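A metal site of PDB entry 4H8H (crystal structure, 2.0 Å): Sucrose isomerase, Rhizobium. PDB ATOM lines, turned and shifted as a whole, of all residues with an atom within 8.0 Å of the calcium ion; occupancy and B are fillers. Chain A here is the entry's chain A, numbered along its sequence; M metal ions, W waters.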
ATOM      1  N   PRO A  17      20.378   4.643  -5.607  1.00  0.00           N
ATOM      2  CA  PRO A  17      20.576   3.367  -4.912  1.00  0.00           C
ATOM      3  C   PRO A  17      21.616   2.475  -5.595  1.00  0.00           C
ATOM      4  O   PRO A  17      22.316   1.745  -4.898  1.00  0.00           O
ATOM      5  CB  PRO A  17      19.190   2.720  -4.964  1.00  0.00           C
ATOM      6  CG  PRO A  17      18.245   3.863  -5.069  1.00  0.00           C
ATOM      7  CD  PRO A  17      18.957   4.865  -5.942  1.00  0.00           C
ATOM      8  N   ARG A  18      21.704   2.528  -6.919  1.00  0.00           N
ATOM      9  CA  ARG A  18      22.628   1.670  -7.668  1.00  0.00           C
ATOM     10  C   ARG A  18      24.090   1.950  -7.312  1.00  0.00           C
ATOM     11  O   ARG A  18      24.947   1.074  -7.434  1.00  0.00           O
ATOM     12  CB  ARG A  18      22.400   1.873  -9.174  1.00  0.00           C
ATOM     13  CG  ARG A  18      23.276   1.002 -10.088  1.00  0.00           C
ATOM     14  CD  ARG A  18      23.083   1.375 -11.575  1.00  0.00           C
ATOM     15  NE  ARG A  18      23.859   0.494 -12.440  1.00  0.00           N
ATOM     16  CZ  ARG A  18      23.420  -0.665 -12.927  1.00  0.00           C
ATOM     17  NH1 ARG A  18      22.201  -1.104 -12.638  1.00  0.00           N
ATOM     18  NH2 ARG A  18      24.210  -1.394 -13.706  1.00  0.00           N
ATOM     19  N   LYS A  21      25.116   1.849  -1.699  1.00  0.00           N
ATOM     20  CA  LYS A  21      25.667   0.836  -0.799  1.00  0.00           C
ATOM     21  C   LYS A  21      25.282  -0.583  -1.204  1.00  0.00           C
ATOM     22  O   LYS A  21      24.099  -0.936  -1.201  1.00  0.00           O
ATOM     23  CB  LYS A  21      25.220   1.107   0.636  1.00  0.00           C
ATOM     24  CG  LYS A  21      25.811   0.123   1.642  1.00  0.00           C
ATOM     25  CD  LYS A  21      27.288   0.404   1.836  1.00  0.00           C
ATOM     26  CE  LYS A  21      28.060  -0.883   1.989  1.00  0.00           C
ATOM     27  NZ  LYS A  21      27.708  -1.613   3.235  1.00  0.00           N
ATOM     28  N   ASP A  22      26.278  -1.410  -1.521  1.00  0.00           N
ATOM     29  CA  ASP A  22      26.024  -2.797  -1.899  1.00  0.00           C
ATOM     30  C   ASP A  22      26.200  -3.722  -0.687  1.00  0.00           C
ATOM     31  O   ASP A  22      27.200  -3.627   0.041  1.00  0.00           O
ATOM     32  CB  ASP A  22      27.003  -3.205  -3.015  1.00  0.00           C
ATOM     33  CG  ASP A  22      26.882  -4.653  -3.419  1.00  0.00           C
ATOM     34  OD1 ASP A  22      25.830  -5.295  -3.150  1.00  0.00           O
ATOM     35  OD2 ASP A  22      27.835  -5.153  -4.044  1.00  0.00           O
ATOM     36  N   THR A  23      25.245  -4.615  -0.474  1.00  0.00           N
ATOM     37  CA  THR A  23      25.316  -5.536   0.665  1.00  0.00           C
ATOM     38  C   THR A  23      25.408  -7.006   0.268  1.00  0.00           C
ATOM     39  O   THR A  23      25.354  -7.880   1.135  1.00  0.00           O
ATOM     40  CB  THR A  23      24.117  -5.368   1.611  1.00  0.00           C
ATOM     41  OG1 THR A  23      22.893  -5.461   0.868  1.00  0.00           O
ATOM     42  CG2 THR A  23      24.166  -4.039   2.307  1.00  0.00           C
ATOM     43  N   ASN A  24      25.521  -7.299  -1.027  1.00  0.00           N
ATOM     44  CA  ASN A  24      25.595  -8.708  -1.433  1.00  0.00           C
ATOM     45  C   ASN A  24      26.658  -9.053  -2.462  1.00  0.00           C
ATOM     46  O   ASN A  24      26.655 -10.156  -3.012  1.00  0.00           O
ATOM     47  CB  ASN A  24      24.228  -9.225  -1.885  1.00  0.00           C
ATOM     48  CG  ASN A  24      23.828  -8.694  -3.250  1.00  0.00           C
ATOM     49  OD1 ASN A  24      24.300  -7.635  -3.677  1.00  0.00           O
ATOM     50  ND2 ASN A  24      22.965  -9.424  -3.930  1.00  0.00           N
ATOM     51  N   GLY A  25      27.560  -8.115  -2.738  1.00  0.00           N
ATOM     52  CA  GLY A  25      28.739  -8.412  -3.535  1.00  0.00           C
ATOM     53  C   GLY A  25      28.553  -8.480  -5.041  1.00  0.00           C
ATOM     54  O   GLY A  25      29.483  -8.879  -5.753  1.00  0.00           O
ATOM     55  N   ASP A  26      27.382  -8.085  -5.548  1.00  0.00           N
ATOM     56  CA  ASP A  26      27.158  -8.111  -6.995  1.00  0.00           C
ATOM     57  C   ASP A  26      27.613  -6.811  -7.664  1.00  0.00           C
ATOM     58  O   ASP A  26      27.547  -6.676  -8.889  1.00  0.00           O
ATOM     59  CB  ASP A  26      25.683  -8.415  -7.329  1.00  0.00           C
ATOM     60  CG  ASP A  26      24.745  -7.252  -7.015  1.00  0.00           C
ATOM     61  OD1 ASP A  26      25.116  -6.345  -6.220  1.00  0.00           O
ATOM     62  OD2 ASP A  26      23.624  -7.244  -7.558  1.00  0.00           O
ATOM     63  N   GLY A  27      28.061  -5.853  -6.844  1.00  0.00           N
ATOM     64  CA  GLY A  27      28.649  -4.630  -7.330  1.00  0.00           C
ATOM     65  C   GLY A  27      27.657  -3.499  -7.528  1.00  0.00           C
ATOM     66  O   GLY A  27      28.025  -2.385  -7.939  1.00  0.00           O
ATOM     67  N   ILE A  28      26.397  -3.769  -7.230  1.00  0.00           N
ATOM     68  CA  ILE A  28      25.351  -2.775  -7.395  1.00  0.00           C
ATOM     69  C   ILE A  28      24.698  -2.471  -6.052  1.00  0.00           C
ATOM     70  O   ILE A  28      24.401  -3.384  -5.274  1.00  0.00           O
ATOM     71  CB  ILE A  28      24.314  -3.259  -8.426  1.00  0.00           C
ATOM     72  CG1 ILE A  28      24.956  -3.316  -9.813  1.00  0.00           C
ATOM     73  CG2 ILE A  28      23.089  -2.341  -8.441  1.00  0.00           C
ATOM     74  CD1 ILE A  28      24.168  -4.110 -10.858  1.00  0.00           C
ATOM     75  N   GLY A  29      24.493  -1.183  -5.767  1.00  0.00           N
ATOM     76  CA  GLY A  29      23.852  -0.795  -4.534  1.00  0.00           C
ATOM     77  C   GLY A  29      22.433  -1.314  -4.488  1.00  0.00           C
ATOM     78  O   GLY A  29      21.797  -1.517  -5.536  1.00  0.00           O
ATOM     79  N   ASP A  30      21.914  -1.512  -3.282  1.00  0.00           N
ATOM     80  CA  ASP A  30      20.604  -2.124  -3.100  1.00  0.00           C
ATOM     81  C   ASP A  30      19.873  -1.470  -1.927  1.00  0.00           C
ATOM     82  O   ASP A  30      20.411  -0.591  -1.248  1.00  0.00           O
ATOM     83  CB  ASP A  30      20.776  -3.626  -2.874  1.00  0.00           C
ATOM     84  CG  ASP A  30      21.910  -3.937  -1.905  1.00  0.00           C
ATOM     85  OD1 ASP A  30      21.754  -3.614  -0.710  1.00  0.00           O
ATOM     86  OD2 ASP A  30      22.937  -4.498  -2.328  1.00  0.00           O
ATOM     87  N   PHE A  31      18.633  -1.905  -1.674  1.00  0.00           N
ATOM     88  CA  PHE A  31      17.820  -1.321  -0.620  1.00  0.00           C
ATOM     89  C   PHE A  31      18.355  -1.598   0.775  1.00  0.00           C
ATOM     90  O   PHE A  31      18.319  -0.730   1.667  1.00  0.00           O
ATOM     91  CB  PHE A  31      16.390  -1.853  -0.719  1.00  0.00           C
ATOM     92  CG  PHE A  31      15.534  -1.096  -1.691  1.00  0.00           C
ATOM     93  CD1 PHE A  31      15.802   0.232  -1.996  1.00  0.00           C
ATOM     94  CD2 PHE A  31      14.462  -1.712  -2.306  1.00  0.00           C
ATOM     95  CE1 PHE A  31      15.015   0.932  -2.890  1.00  0.00           C
ATOM     96  CE2 PHE A  31      13.666  -1.023  -3.199  1.00  0.00           C
ATOM     97  CZ  PHE A  31      13.942   0.293  -3.476  1.00  0.00           C
ATOM     98  N   LYS A  32      18.828  -2.825   0.993  1.00  0.00           N
ATOM     99  CA  LYS A  32      19.345  -3.164   2.312  1.00  0.00           C
ATOM    100  C   LYS A  32      20.600  -2.335   2.643  1.00  0.00           C
ATOM    101  O   LYS A  32      20.839  -2.000   3.794  1.00  0.00           O
ATOM    102  CB  LYS A  32      19.574  -4.663   2.448  1.00  0.00           C
ATOM    103  CG  LYS A  32      18.248  -5.404   2.611  1.00  0.00           C
ATOM    104  CD  LYS A  32      18.424  -6.871   2.966  1.00  0.00           C
ATOM    105  CE  LYS A  32      18.683  -7.710   1.736  1.00  0.00           C
ATOM    106  NZ  LYS A  32      18.464  -9.156   2.034  1.00  0.00           N
ATOM    107  N   GLY A  33      21.367  -1.986   1.609  1.00  0.00           N
ATOM    108  CA  GLY A  33      22.472  -1.066   1.807  1.00  0.00           C
ATOM    109  C   GLY A  33      21.981   0.303   2.239  1.00  0.00           C
ATOM    110  O   GLY A  33      22.514   0.897   3.182  1.00  0.00           O
ATOM    111  N   LYS A  74      14.955  -5.848  -9.455  1.00  0.00           N
ATOM    112  CA  LYS A  74      15.641  -7.027  -8.886  1.00  0.00           C
ATOM    113  C   LYS A  74      16.969  -6.668  -8.219  1.00  0.00           C
ATOM    114  O   LYS A  74      17.294  -7.208  -7.147  1.00  0.00           O
ATOM    115  CB  LYS A  74      15.856  -8.096  -9.970  1.00  0.00           C
ATOM    116  N   GLU A  75      17.748  -5.776  -8.819  1.00  0.00           N
ATOM    117  CA  GLU A  75      19.039  -5.380  -8.231  1.00  0.00           C
ATOM    118  C   GLU A  75      18.894  -4.747  -6.848  1.00  0.00           C
ATOM    119  O   GLU A  75      19.817  -4.807  -6.030  1.00  0.00           O
ATOM    120  CB  GLU A  75      19.799  -4.438  -9.167  1.00  0.00           C
ATOM    121  CG  GLU A  75      20.487  -5.123 -10.351  1.00  0.00           C
ATOM    122  CD  GLU A  75      19.514  -5.461 -11.481  1.00  0.00           C
ATOM    123  OE1 GLU A  75      18.337  -5.067 -11.398  1.00  0.00           O
ATOM    124  OE2 GLU A  75      19.937  -6.121 -12.457  1.00  0.00           O
ATOM    125  N   TYR A  76      17.746  -4.133  -6.572  1.00  0.00           N
ATOM    126  CA  TYR A  76      17.611  -3.404  -5.308  1.00  0.00           C
ATOM    127  C   TYR A  76      17.049  -4.251  -4.169  1.00  0.00           C
ATOM    128  O   TYR A  76      17.287  -3.950  -2.991  1.00  0.00           O
ATOM    129  CB  TYR A  76      16.796  -2.125  -5.501  1.00  0.00           C
ATOM    130  CG  TYR A  76      17.420  -1.145  -6.465  1.00  0.00           C
ATOM    131  CD1 TYR A  76      18.756  -1.263  -6.860  1.00  0.00           C
ATOM    132  CD2 TYR A  76      16.673  -0.085  -6.986  1.00  0.00           C
ATOM    133  CE1 TYR A  76      19.326  -0.366  -7.743  1.00  0.00           C
ATOM    134  CE2 TYR A  76      17.237   0.824  -7.888  1.00  0.00           C
ATOM    135  CZ  TYR A  76      18.560   0.683  -8.260  1.00  0.00           C
ATOM    136  OH  TYR A  76      19.120   1.579  -9.140  1.00  0.00           O
ATOM    137  N   GLY A  77      16.328  -5.308  -4.518  1.00  0.00           N
ATOM    138  CA  GLY A  77      15.748  -6.199  -3.526  1.00  0.00           C
ATOM    139  C   GLY A  77      14.334  -6.660  -3.874  1.00  0.00           C
ATOM    140  O   GLY A  77      13.990  -6.795  -5.045  1.00  0.00           O
ATOM    141  N   PHE A 431      32.189   0.362  -0.528  1.00  0.00           N
ATOM    142  CA  PHE A 431      30.910   0.342  -1.226  1.00  0.00           C
ATOM    143  C   PHE A 431      30.448  -1.085  -1.504  1.00  0.00           C
ATOM    144  O   PHE A 431      29.257  -1.395  -1.441  1.00  0.00           O
ATOM    145  CB  PHE A 431      30.974   1.120  -2.547  1.00  0.00           C
ATOM    146  CG  PHE A 431      29.862   0.766  -3.510  1.00  0.00           C
ATOM    147  CD1 PHE A 431      28.577   1.252  -3.312  1.00  0.00           C
ATOM    148  CD2 PHE A 431      30.105  -0.039  -4.605  1.00  0.00           C
ATOM    149  CE1 PHE A 431      27.552   0.931  -4.182  1.00  0.00           C
ATOM    150  CE2 PHE A 431      29.097  -0.357  -5.491  1.00  0.00           C
ATOM    151  CZ  PHE A 431      27.815   0.128  -5.283  1.00  0.00           C
ATOM    152  N   THR A 432      31.402  -1.963  -1.834  1.00  0.00           N
ATOM    153  CA  THR A 432      31.057  -3.349  -2.163  1.00  0.00           C
ATOM    154  C   THR A 432      32.153  -4.311  -1.747  1.00  0.00           C
ATOM    155  O   THR A 432      33.307  -3.918  -1.591  1.00  0.00           O
ATOM    156  CB  THR A 432      30.759  -3.500  -3.686  1.00  0.00           C
ATOM    157  OG1 THR A 432      30.402  -4.851  -3.977  1.00  0.00           O
ATOM    158  CG2 THR A 432      31.982  -3.117  -4.507  1.00  0.00           C
HETATM  159 CA    CA M   1      23.763  -5.482  -4.406  1.00  0.00          CA
HETATM  160  O   HOH W   1      22.445  -5.391  -6.204  1.00  0.00           O
HETATM  161  O   HOH W   2      21.363  -6.863  -3.831  1.00  0.00           O
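The side-chain carboxylate of Asp 22 sits at hydrogen-bond distance from the side-chain hydroxyl of Thr 432 (2.6 Å). The side-chain carboxylate (OD2) of Asp 22 is in hydrogen-bond range of the backbone NH (N) of Gly 27, 2.9 Å away. The backbone NH (N) of Gly 33 sits at hydrogen-bond distance from the side-chain carboxylate (OD1) of Asp 30. The backbone NH (N) of Gly 25 lies within hydrogen-bond range of the side-chain carboxylate (OD2) of Asp 22 (3.2 Å). The side-chain carboxylate (OD1) of Asp 30 lies within hydrogen-bond range of the side-chain hydroxyl (OG1) of Thr 23, at 2.7 Å. OD1 of Asp 30 lies close to N of Lys 32 (3.5 Å). The backbone NH (N) of Asp 30 lies within hydrogen-bond range of the backbone carbonyl oxygen (O) of Lys 21 (3.1 Å). O of Phe 431 lies within hydrogen-bond range of N of Asp 22.
Five residues have an atom within 4 Å of the calcium ion: Asp 22, Asn 24, Asp 26, Ile 28 and Asp 30. The nearest printed residue that does not touch the calcium ion is Thr 23 (4.3 Å).
The calcium ion is bound by water W1, OD1 of Asn 24, O of Ile 28, OD1 of Asp 26, OD1 of Asp 22, OD2 of Asp 30 and water W2. The calcium ion has seven donor atoms within binding distance.
Water W1 lies within hydrogen-bond range of the side-chain carboxylate (OD2) of Asp 26 (2.6 Å) and the backbone carbonyl oxygen (O) of Glu 75 (2.7 Å). Water W2 bridges ND2 of Asn 24 and O of Glu 75.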
